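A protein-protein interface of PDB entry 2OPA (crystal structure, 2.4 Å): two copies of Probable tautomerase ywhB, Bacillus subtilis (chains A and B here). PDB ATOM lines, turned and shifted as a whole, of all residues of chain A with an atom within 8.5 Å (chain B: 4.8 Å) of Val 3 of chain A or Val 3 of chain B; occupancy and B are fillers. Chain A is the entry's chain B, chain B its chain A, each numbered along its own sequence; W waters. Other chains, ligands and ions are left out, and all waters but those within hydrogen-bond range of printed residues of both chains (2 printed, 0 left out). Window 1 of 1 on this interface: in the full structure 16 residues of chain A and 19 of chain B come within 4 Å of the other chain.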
ATOM      1  N   PRO A   1      16.571  -7.087 -22.634  1.00  0.00           N
ATOM      2  CA  PRO A   1      16.464  -5.621 -22.825  1.00  0.00           C
ATOM      3  C   PRO A   1      16.991  -5.123 -24.163  1.00  0.00           C
ATOM      4  O   PRO A   1      17.788  -5.791 -24.820  1.00  0.00           O
ATOM      5  CB  PRO A   1      17.203  -4.952 -21.671  1.00  0.00           C
ATOM      6  CG  PRO A   1      17.976  -6.115 -21.064  1.00  0.00           C
ATOM      7  CD  PRO A   1      17.134  -7.366 -21.308  1.00  0.00           C
ATOM      8  N   TYR A   2      16.528  -3.939 -24.552  1.00  0.00           N
ATOM      9  CA  TYR A   2      16.909  -3.313 -25.808  1.00  0.00           C
ATOM     10  C   TYR A   2      17.605  -2.005 -25.535  1.00  0.00           C
ATOM     11  O   TYR A   2      17.042  -1.102 -24.909  1.00  0.00           O
ATOM     12  CB  TYR A   2      15.683  -3.052 -26.668  1.00  0.00           C
ATOM     13  CG  TYR A   2      14.922  -4.306 -26.967  1.00  0.00           C
ATOM     14  CD1 TYR A   2      13.948  -4.784 -26.086  1.00  0.00           C
ATOM     15  CD2 TYR A   2      15.217  -5.054 -28.099  1.00  0.00           C
ATOM     16  CE1 TYR A   2      13.287  -5.982 -26.333  1.00  0.00           C
ATOM     17  CE2 TYR A   2      14.570  -6.248 -28.354  1.00  0.00           C
ATOM     18  CZ  TYR A   2      13.608  -6.710 -27.471  1.00  0.00           C
ATOM     19  OH  TYR A   2      12.979  -7.905 -27.739  1.00  0.00           O
ATOM     20  N   VAL A   3      18.837  -1.911 -26.012  1.00  0.00           N
ATOM     21  CA  VAL A   3      19.637  -0.723 -25.816  1.00  0.00           C
ATOM     22  C   VAL A   3      19.920  -0.052 -27.139  1.00  0.00           C
ATOM     23  O   VAL A   3      20.404  -0.686 -28.079  1.00  0.00           O
ATOM     24  CB  VAL A   3      20.987  -1.065 -25.161  1.00  0.00           C
ATOM     25  CG1 VAL A   3      21.742   0.211 -24.839  1.00  0.00           C
ATOM     26  CG2 VAL A   3      20.763  -1.904 -23.911  1.00  0.00           C
ATOM     27  N   THR A   4      19.601   1.231 -27.214  1.00  0.00           N
ATOM     28  CA  THR A   4      19.874   1.992 -28.412  1.00  0.00           C
ATOM     29  C   THR A   4      20.921   3.032 -28.021  1.00  0.00           C
ATOM     30  O   THR A   4      20.733   3.788 -27.063  1.00  0.00           O
ATOM     31  CB  THR A   4      18.612   2.718 -28.941  1.00  0.00           C
ATOM     32  OG1 THR A   4      17.620   1.751 -29.296  1.00  0.00           O
ATOM     33  CG2 THR A   4      18.946   3.552 -30.180  1.00  0.00           C
ATOM     34  N   VAL A   5      22.044   3.034 -28.731  1.00  0.00           N
ATOM     35  CA  VAL A   5      23.092   4.011 -28.479  1.00  0.00           C
ATOM     36  C   VAL A   5      23.067   4.945 -29.681  1.00  0.00           C
ATOM     37  O   VAL A   5      23.293   4.513 -30.811  1.00  0.00           O
ATOM     38  CB  VAL A   5      24.487   3.361 -28.388  1.00  0.00           C
ATOM     39  CG1 VAL A   5      25.533   4.427 -28.056  1.00  0.00           C
ATOM     40  CG2 VAL A   5      24.493   2.274 -27.326  1.00  0.00           C
ATOM     41  N   LYS A   6      22.757   6.214 -29.440  1.00  0.00           N
ATOM     42  CA  LYS A   6      22.704   7.207 -30.507  1.00  0.00           C
ATOM     43  C   LYS A   6      23.914   8.120 -30.347  1.00  0.00           C
ATOM     44  O   LYS A   6      24.047   8.809 -29.336  1.00  0.00           O
ATOM     45  CB  LYS A   6      21.404   8.023 -30.412  1.00  0.00           C
ATOM     46  CG  LYS A   6      21.184   8.968 -31.577  1.00  0.00           C
ATOM     47  CD  LYS A   6      19.782   9.567 -31.595  1.00  0.00           C
ATOM     48  CE  LYS A   6      19.556  10.330 -32.905  1.00  0.00           C
ATOM     49  NZ  LYS A   6      18.217  10.987 -33.012  1.00  0.00           N
ATOM     50  N   MET A   7      24.802   8.114 -31.336  1.00  0.00           N
ATOM     51  CA  MET A   7      26.005   8.938 -31.271  1.00  0.00           C
ATOM     52  C   MET A   7      26.424   9.468 -32.639  1.00  0.00           C
ATOM     53  O   MET A   7      25.979   8.974 -33.677  1.00  0.00           O
ATOM     54  CB  MET A   7      27.157   8.134 -30.652  1.00  0.00           C
ATOM     55  CG  MET A   7      27.557   6.928 -31.469  1.00  0.00           C
ATOM     56  SD  MET A   7      28.817   5.892 -30.710  1.00  0.00           S
ATOM     57  CE  MET A   7      28.967   4.621 -31.954  1.00  0.00           C
ATOM     58  N   LEU A  19      31.891  -1.322 -28.050  1.00  0.00           N
ATOM     59  CA  LEU A  19      30.722  -0.670 -27.472  1.00  0.00           C
ATOM     60  C   LEU A  19      29.632  -1.706 -27.224  1.00  0.00           C
ATOM     61  O   LEU A  19      29.066  -1.778 -26.143  1.00  0.00           O
ATOM     62  CB  LEU A  19      30.192   0.409 -28.419  1.00  0.00           C
ATOM     63  CG  LEU A  19      28.833   1.021 -28.061  1.00  0.00           C
ATOM     64  CD1 LEU A  19      28.894   1.657 -26.685  1.00  0.00           C
ATOM     65  CD2 LEU A  19      28.445   2.046 -29.107  1.00  0.00           C
ATOM     66  N   VAL A  20      29.359  -2.509 -28.243  1.00  0.00           N
ATOM     67  CA  VAL A  20      28.351  -3.547 -28.167  1.00  0.00           C
ATOM     68  C   VAL A  20      28.656  -4.569 -27.078  1.00  0.00           C
ATOM     69  O   VAL A  20      27.765  -4.970 -26.320  1.00  0.00           O
ATOM     70  CB  VAL A  20      28.220  -4.271 -29.530  1.00  0.00           C
ATOM     71  CG1 VAL A  20      27.572  -5.632 -29.349  1.00  0.00           C
ATOM     72  CG2 VAL A  20      27.388  -3.426 -30.479  1.00  0.00           C
ATOM     73  N   VAL A  23      28.658  -2.725 -23.415  1.00  0.00           N
ATOM     74  CA  VAL A  23      27.298  -2.354 -23.056  1.00  0.00           C
ATOM     75  C   VAL A  23      26.473  -3.593 -22.722  1.00  0.00           C
ATOM     76  O   VAL A  23      25.692  -3.580 -21.776  1.00  0.00           O
ATOM     77  CB  VAL A  23      26.622  -1.539 -24.184  1.00  0.00           C
ATOM     78  CG1 VAL A  23      25.111  -1.555 -24.021  1.00  0.00           C
ATOM     79  CG2 VAL A  23      27.121  -0.106 -24.135  1.00  0.00           C
ATOM     80  N   THR A  24      26.657  -4.667 -23.485  1.00  0.00           N
ATOM     81  CA  THR A  24      25.926  -5.899 -23.223  1.00  0.00           C
ATOM     82  C   THR A  24      26.304  -6.465 -21.857  1.00  0.00           C
ATOM     83  O   THR A  24      25.449  -6.936 -21.115  1.00  0.00           O
ATOM     84  CB  THR A  24      26.206  -6.965 -24.290  1.00  0.00           C
ATOM     85  OG1 THR A  24      25.682  -6.530 -25.552  1.00  0.00           O
ATOM     86  CG2 THR A  24      25.556  -8.287 -23.898  1.00  0.00           C
ATOM     87  N   ALA A  26      27.439  -4.753 -19.305  1.00  0.00           N
ATOM     88  CA  ALA A  26      26.922  -3.844 -18.290  1.00  0.00           C
ATOM     89  C   ALA A  26      25.462  -4.181 -17.995  1.00  0.00           C
ATOM     90  O   ALA A  26      25.049  -4.234 -16.839  1.00  0.00           O
ATOM     91  CB  ALA A  26      27.051  -2.395 -18.762  1.00  0.00           C
ATOM     92  N   VAL A  27      24.682  -4.421 -19.043  1.00  0.00           N
ATOM     93  CA  VAL A  27      23.275  -4.756 -18.869  1.00  0.00           C
ATOM     94  C   VAL A  27      23.123  -6.103 -18.161  1.00  0.00           C
ATOM     95  O   VAL A  27      22.370  -6.220 -17.191  1.00  0.00           O
ATOM     96  CB  VAL A  27      22.534  -4.805 -20.233  1.00  0.00           C
ATOM     97  CG1 VAL A  27      21.121  -5.361 -20.052  1.00  0.00           C
ATOM     98  CG2 VAL A  27      22.471  -3.412 -20.838  1.00  0.00           C
ATOM     99  N   LYS A  28      23.846  -7.114 -18.641  1.00  0.00           N
ATOM    100  CA  LYS A  28      23.779  -8.450 -18.048  1.00  0.00           C
ATOM    101  C   LYS A  28      24.101  -8.470 -16.554  1.00  0.00           C
ATOM    102  O   LYS A  28      23.378  -9.067 -15.761  1.00  0.00           O
ATOM    103  CB  LYS A  28      24.741  -9.403 -18.759  1.00  0.00           C
ATOM    104  CG  LYS A  28      24.836 -10.758 -18.077  1.00  0.00           C
ATOM    105  CD  LYS A  28      26.268 -11.278 -18.039  1.00  0.00           C
ATOM    106  CE  LYS A  28      26.575 -12.195 -19.213  1.00  0.00           C
ATOM    107  NZ  LYS A  28      25.782 -13.451 -19.150  1.00  0.00           N
ATOM    108  N   THR A  31      21.240  -6.101 -14.510  1.00  0.00           N
ATOM    109  CA  THR A  31      19.808  -6.386 -14.528  1.00  0.00           C
ATOM    110  C   THR A  31      19.499  -7.873 -14.392  1.00  0.00           C
ATOM    111  O   THR A  31      18.353  -8.258 -14.147  1.00  0.00           O
ATOM    112  CB  THR A  31      19.157  -5.897 -15.835  1.00  0.00           C
ATOM    113  OG1 THR A  31      19.556  -6.750 -16.914  1.00  0.00           O
ATOM    114  CG2 THR A  31      19.576  -4.470 -16.142  1.00  0.00           C
ATOM    115  N   LYS A  37      19.168 -12.350 -24.569  1.00  0.00           N
ATOM    116  CA  LYS A  37      17.974 -11.523 -24.456  1.00  0.00           C
ATOM    117  C   LYS A  37      18.359 -10.043 -24.454  1.00  0.00           C
ATOM    118  O   LYS A  37      17.512  -9.177 -24.237  1.00  0.00           O
ATOM    119  CB  LYS A  37      17.209 -11.876 -23.181  1.00  0.00           C
ATOM    120  N   ILE A  38      19.639  -9.764 -24.697  1.00  0.00           N
ATOM    121  CA  ILE A  38      20.151  -8.399 -24.724  1.00  0.00           C
ATOM    122  C   ILE A  38      20.478  -7.961 -26.150  1.00  0.00           C
ATOM    123  O   ILE A  38      21.429  -8.450 -26.761  1.00  0.00           O
ATOM    124  CB  ILE A  38      21.424  -8.268 -23.880  1.00  0.00           C
ATOM    125  CG1 ILE A  38      21.141  -8.703 -22.444  1.00  0.00           C
ATOM    126  CG2 ILE A  38      21.933  -6.827 -23.923  1.00  0.00           C
ATOM    127  CD1 ILE A  38      22.371  -8.701 -21.552  1.00  0.00           C
ATOM    128  N   VAL A  39      19.686  -7.027 -26.666  1.00  0.00           N
ATOM    129  CA  VAL A  39      19.851  -6.511 -28.016  1.00  0.00           C
ATOM    130  C   VAL A  39      20.377  -5.078 -27.995  1.00  0.00           C
ATOM    131  O   VAL A  39      19.935  -4.263 -27.191  1.00  0.00           O
ATOM    132  CB  VAL A  39      18.507  -6.529 -28.760  1.00  0.00           C
ATOM    133  CG1 VAL A  39      18.662  -5.951 -30.148  1.00  0.00           C
ATOM    134  CG2 VAL A  39      17.983  -7.943 -28.819  1.00  0.00           C
ATOM    135  N   VAL A  40      21.318  -4.776 -28.885  1.00  0.00           N
ATOM    136  CA  VAL A  40      21.884  -3.437 -28.960  1.00  0.00           C
ATOM    137  C   VAL A  40      21.788  -2.837 -30.358  1.00  0.00           C
ATOM    138  O   VAL A  40      22.189  -3.458 -31.340  1.00  0.00           O
ATOM    139  CB  VAL A  40      23.363  -3.434 -28.547  1.00  0.00           C
ATOM    140  CG1 VAL A  40      23.923  -2.024 -28.673  1.00  0.00           C
ATOM    141  CG2 VAL A  40      23.508  -3.951 -27.123  1.00  0.00           C
ATOM    142  N   PHE A  41      21.247  -1.627 -30.444  1.00  0.00           N
ATOM    143  CA  PHE A  41      21.123  -0.931 -31.719  1.00  0.00           C
ATOM    144  C   PHE A  41      22.041   0.282 -31.684  1.00  0.00           C
ATOM    145  O   PHE A  41      22.116   0.982 -30.674  1.00  0.00           O
ATOM    146  CB  PHE A  41      19.704  -0.409 -31.953  1.00  0.00           C
ATOM    147  CG  PHE A  41      18.635  -1.453 -31.891  1.00  0.00           C
ATOM    148  CD1 PHE A  41      18.041  -1.792 -30.676  1.00  0.00           C
ATOM    149  CD2 PHE A  41      18.175  -2.060 -33.054  1.00  0.00           C
ATOM    150  CE1 PHE A  41      16.997  -2.714 -30.630  1.00  0.00           C
ATOM    151  CE2 PHE A  41      17.132  -2.983 -33.011  1.00  0.00           C
ATOM    152  CZ  PHE A  41      16.545  -3.308 -31.801  1.00  0.00           C
ATOM    153  N   ILE A  42      22.738   0.532 -32.782  1.00  0.00           N
ATOM    154  CA  ILE A  42      23.608   1.693 -32.863  1.00  0.00           C
ATOM    155  C   ILE A  42      23.001   2.642 -33.895  1.00  0.00           C
ATOM    156  O   ILE A  42      22.642   2.229 -34.999  1.00  0.00           O
ATOM    157  CB  ILE A  42      25.043   1.314 -33.308  1.00  0.00           C
ATOM    158  CG1 ILE A  42      25.684   0.379 -32.278  1.00  0.00           C
ATOM    159  CG2 ILE A  42      25.881   2.575 -33.480  1.00  0.00           C
ATOM    160  CD1 ILE A  42      27.086  -0.105 -32.660  1.00  0.00           C
ATOM    161  N   GLU A  43      22.861   3.905 -33.521  1.00  0.00           N
ATOM    162  CA  GLU A  43      22.306   4.909 -34.418  1.00  0.00           C
ATOM    163  C   GLU A  43      23.292   6.065 -34.505  1.00  0.00           C
ATOM    164  O   GLU A  43      23.669   6.657 -33.495  1.00  0.00           O
ATOM    165  CB  GLU A  43      20.954   5.407 -33.899  1.00  0.00           C
ATOM    166  CG  GLU A  43      19.816   4.419 -34.097  1.00  0.00           C
ATOM    167  CD  GLU A  43      18.507   4.903 -33.487  1.00  0.00           C
ATOM    168  OE1 GLU A  43      18.366   6.126 -33.261  1.00  0.00           O
ATOM    169  OE2 GLU A  43      17.613   4.060 -33.246  1.00  0.00           O
ATOM    170  N   PRO B   1      26.720  11.043 -26.377  1.00  0.00           N
ATOM    171  CA  PRO B   1      25.975   9.809 -26.729  1.00  0.00           C
ATOM    172  C   PRO B   1      24.708   9.627 -25.886  1.00  0.00           C
ATOM    173  O   PRO B   1      24.731   9.795 -24.663  1.00  0.00           O
ATOM    174  CB  PRO B   1      26.935   8.647 -26.527  1.00  0.00           C
ATOM    175  CG  PRO B   1      28.290   9.340 -26.772  1.00  0.00           C
ATOM    176  CD  PRO B   1      28.131  10.717 -26.109  1.00  0.00           C
ATOM    177  N   TYR B   2      23.607   9.290 -26.555  1.00  0.00           N
ATOM    178  CA  TYR B   2      22.329   9.079 -25.889  1.00  0.00           C
ATOM    179  C   TYR B   2      21.977   7.606 -25.869  1.00  0.00           C
ATOM    180  O   TYR B   2      21.807   6.978 -26.915  1.00  0.00           O
ATOM    181  CB  TYR B   2      21.230   9.876 -26.589  1.00  0.00           C
ATOM    182  CG  TYR B   2      21.502  11.351 -26.550  1.00  0.00           C
ATOM    183  CD1 TYR B   2      22.384  11.938 -27.458  1.00  0.00           C
ATOM    184  CD2 TYR B   2      20.960  12.149 -25.543  1.00  0.00           C
ATOM    185  CE1 TYR B   2      22.728  13.283 -27.363  1.00  0.00           C
ATOM    186  CE2 TYR B   2      21.299  13.498 -25.437  1.00  0.00           C
ATOM    187  CZ  TYR B   2      22.184  14.056 -26.349  1.00  0.00           C
ATOM    188  OH  TYR B   2      22.529  15.382 -26.237  1.00  0.00           O
ATOM    189  N   VAL B   3      21.874   7.058 -24.666  1.00  0.00           N
ATOM    190  CA  VAL B   3      21.562   5.651 -24.507  1.00  0.00           C
ATOM    191  C   VAL B   3      20.170   5.443 -23.933  1.00  0.00           C
ATOM    192  O   VAL B   3      19.842   5.955 -22.864  1.00  0.00           O
ATOM    193  CB  VAL B   3      22.587   4.962 -23.580  1.00  0.00           C
ATOM    194  CG1 VAL B   3      22.243   3.495 -23.420  1.00  0.00           C
ATOM    195  CG2 VAL B   3      23.990   5.119 -24.152  1.00  0.00           C
ATOM    196  N   THR B   4      19.349   4.700 -24.664  1.00  0.00           N
ATOM    197  CA  THR B   4      18.004   4.387 -24.225  1.00  0.00           C
ATOM    198  C   THR B   4      17.982   2.893 -23.905  1.00  0.00           C
ATOM    199  O   THR B   4      18.292   2.064 -24.759  1.00  0.00           O
ATOM    200  CB  THR B   4      16.961   4.681 -25.331  1.00  0.00           C
ATOM    201  OG1 THR B   4      16.996   6.072 -25.661  1.00  0.00           O
ATOM    202  CG2 THR B   4      15.548   4.331 -24.851  1.00  0.00           C
ATOM    203  N   VAL B   5      17.644   2.555 -22.667  1.00  0.00           N
ATOM    204  CA  VAL B   5      17.561   1.159 -22.266  1.00  0.00           C
ATOM    205  C   VAL B   5      16.095   0.839 -22.075  1.00  0.00           C
ATOM    206  O   VAL B   5      15.454   1.365 -21.170  1.00  0.00           O
ATOM    207  CB  VAL B   5      18.294   0.879 -20.929  1.00  0.00           C
ATOM    208  CG1 VAL B   5      18.201  -0.600 -20.600  1.00  0.00           C
ATOM    209  CG2 VAL B   5      19.745   1.301 -21.018  1.00  0.00           C
ATOM    210  N   VAL B  23      26.529   1.239 -17.706  1.00  0.00           N
ATOM    211  CA  VAL B  23      26.321   1.551 -19.118  1.00  0.00           C
ATOM    212  C   VAL B  23      27.075   2.823 -19.506  1.00  0.00           C
ATOM    213  O   VAL B  23      27.699   2.888 -20.569  1.00  0.00           O
ATOM    214  CB  VAL B  23      24.806   1.726 -19.435  1.00  0.00           C
ATOM    215  CG1 VAL B  23      24.608   2.388 -20.802  1.00  0.00           C
ATOM    216  CG2 VAL B  23      24.124   0.373 -19.425  1.00  0.00           C
ATOM    217  N   VAL B  27      30.173   3.001 -22.284  1.00  0.00           N
ATOM    218  CA  VAL B  27      30.164   3.929 -23.411  1.00  0.00           C
ATOM    219  C   VAL B  27      31.400   4.821 -23.383  1.00  0.00           C
ATOM    220  O   VAL B  27      32.049   5.038 -24.407  1.00  0.00           O
ATOM    221  CB  VAL B  27      28.894   4.831 -23.384  1.00  0.00           C
ATOM    222  CG1 VAL B  27      29.008   5.950 -24.417  1.00  0.00           C
ATOM    223  CG2 VAL B  27      27.661   3.992 -23.661  1.00  0.00           C
ATOM    224  N   VAL B  39      24.324  10.507 -21.841  1.00  0.00           N
ATOM    225  CA  VAL B  39      22.986  10.552 -21.281  1.00  0.00           C
ATOM    226  C   VAL B  39      22.323   9.183 -21.382  1.00  0.00           C
ATOM    227  O   VAL B  39      22.445   8.502 -22.406  1.00  0.00           O
ATOM    228  CB  VAL B  39      22.129  11.581 -22.037  1.00  0.00           C
ATOM    229  CG1 VAL B  39      20.670  11.509 -21.580  1.00  0.00           C
ATOM    230  CG2 VAL B  39      22.700  12.973 -21.816  1.00  0.00           C
ATOM    231  N   VAL B  40      21.631   8.785 -20.318  1.00  0.00           N
ATOM    232  CA  VAL B  40      20.942   7.506 -20.307  1.00  0.00           C
ATOM    233  C   VAL B  40      19.457   7.663 -19.964  1.00  0.00           C
ATOM    234  O   VAL B  40      19.100   8.340 -18.997  1.00  0.00           O
ATOM    235  CB  VAL B  40      21.583   6.524 -19.293  1.00  0.00           C
ATOM    236  CG1 VAL B  40      20.858   5.191 -19.329  1.00  0.00           C
ATOM    237  CG2 VAL B  40      23.052   6.327 -19.613  1.00  0.00           C
ATOM    238  N   PHE B  41      18.603   7.045 -20.776  1.00  0.00           N
ATOM    239  CA  PHE B  41      17.165   7.077 -20.547  1.00  0.00           C
ATOM    240  C   PHE B  41      16.733   5.649 -20.273  1.00  0.00           C
ATOM    241  O   PHE B  41      17.166   4.729 -20.964  1.00  0.00           O
ATOM    242  CB  PHE B  41      16.386   7.553 -21.783  1.00  0.00           C
ATOM    243  CG  PHE B  41      16.798   8.896 -22.303  1.00  0.00           C
ATOM    244  CD1 PHE B  41      17.619   9.001 -23.425  1.00  0.00           C
ATOM    245  CD2 PHE B  41      16.341  10.063 -21.697  1.00  0.00           C
ATOM    246  CE1 PHE B  41      17.973  10.253 -23.941  1.00  0.00           C
ATOM    247  CE2 PHE B  41      16.690  11.315 -22.204  1.00  0.00           C
ATOM    248  CZ  PHE B  41      17.506  11.407 -23.327  1.00  0.00           C
HETATM  249  O   HOH W   1      16.231   1.081 -27.052  1.00  0.00           O
HETATM  250  O   HOH W   2      19.066   6.525 -27.340  1.00  0.00           O
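Of the 22 printed residues of chain A, 6 touch a printed residue of chain B. Printed residues of chain A that touch a printed residue of chain B: Tyr 2, Val 3, Thr 4, Val 5, Lys 6 and Ala 26. Hydrophobic or aromatic side chains of chain B that line the printed part of chain A: Val 3. Among the printed residues, 11 pairs touch across the chains.
The backbone NH (N) of Lys 6 of chain A sits at hydrogen-bond distance from the backbone carbonyl oxygen (O) of Tyr 2 of chain B (2.8 Å). The backbone carbonyl oxygen of Thr 4 of chain B sits at hydrogen-bond distance from the backbone NH of Thr 4 of chain A. O of Tyr 2 of chain A lies close to O of Thr 4 of chain B (3.4 Å). The backbone carbonyl oxygen (O) of Tyr 2 of chain B lies close to the backbone carbonyl oxygen (O) of Thr 4 of chain A, 3.4 Å away.
Tyr 2 of chain A touches Thr 4 of chain B, and with the chains exchanged Thr 4 of chain A touches Tyr 2 of chain B. Val 3 of chain A touches its own counterpart, Val 3 of chain B. Val 3 of chain A touches Thr 4 of chain B, and with the chains exchanged Thr 4 of chain A touches Val 3 of chain B. Thr 4 of chain A touches its own counterpart, Thr 4 of chain B. 10 positions are printed for both chains.
Water W2 lies within hydrogen-bond range of OG1 of Thr 4 of chain B (2.7 Å), O of Tyr 2 of chain B (2.8 Å) and O of Thr 4 of chain A (3.2 Å). Water W1 lies within hydrogen-bond range of the side-chain hydroxyl of Thr 4 of chain A, the backbone carbonyl oxygen of Tyr 2 of chain A and the backbone carbonyl oxygen of Thr 4 of chain B.
Tyr 2 of chain A touches Val 5 of chain B. Val 3 of chain B touches Val 3 of chain A (CG1 to CG1, 3.6 Å). Thr 4 of chain B touches Val 3 of chain A (O to CA, 3.3 Å). Val 3 of chain B touches Thr 4 of chain A. CA of Val 5 of chain A touches O of Tyr 2 of chain B, 3.6 Å away. O of Lys 6 of chain A touches CA of Pro 1 of chain B, 3.4 Å away. N of Val 23 of chain B touches CB of Ala 26 of chain A, at 3.8 Å.
Val 3 of chain A touches just these residues of chain B: Val 3 (3.6 Å) and Thr 4 (3.3 Å). Printed residues of chain B within 4 Å of Thr 4 of chain A: Tyr 2, Val 3 and Thr 4. Printed residues of chain B within 4 Å of Lys 6 of chain A: Pro 1 (3.4 Å) and Tyr 2 (2.8 Å). Val 27 of chain A touches none of the printed residues of chain B. Val 3 of chain B touches just these residues of chain A: Val 3 (3.6 Å) and Thr 4 (3.3 Å). Of the printed residues of chain A, Val 23 of chain B touches Ala 26. The nearest residue of chain A that does not touch Val 3 of chain B is Val 5 of chain A (4.3 Å). The nearest printed residue of chain B that does not touch Tyr 2 of chain A is Phe 41 of chain B (7.0 Å).
The backbone carbonyl oxygen (O) of Val 39 of chain B is in hydrogen-bond range of the backbone NH (N) of Val 3 of chain B (2.7 Å). The backbone carbonyl oxygen (O) of Val 3 of chain B sits at hydrogen-bond distance from the backbone NH (N) of Phe 41 of chain B, at 2.7 Å. The backbone NH (N) of Val 5 of chain B sits at hydrogen-bond distance from the backbone carbonyl oxygen (O) of Phe 41 of chain B (2.8 Å). O of Val 39 of chain A lies within hydrogen-bond range of N of Val 3 of chain A (2.9 Å). O of Val 3 of chain A lies within hydrogen-bond range of N of Phe 41 of chain A, 2.7 Å away. O of Phe 41 of chain A lies within hydrogen-bond range of N of Val 5 of chain A (2.8 Å).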
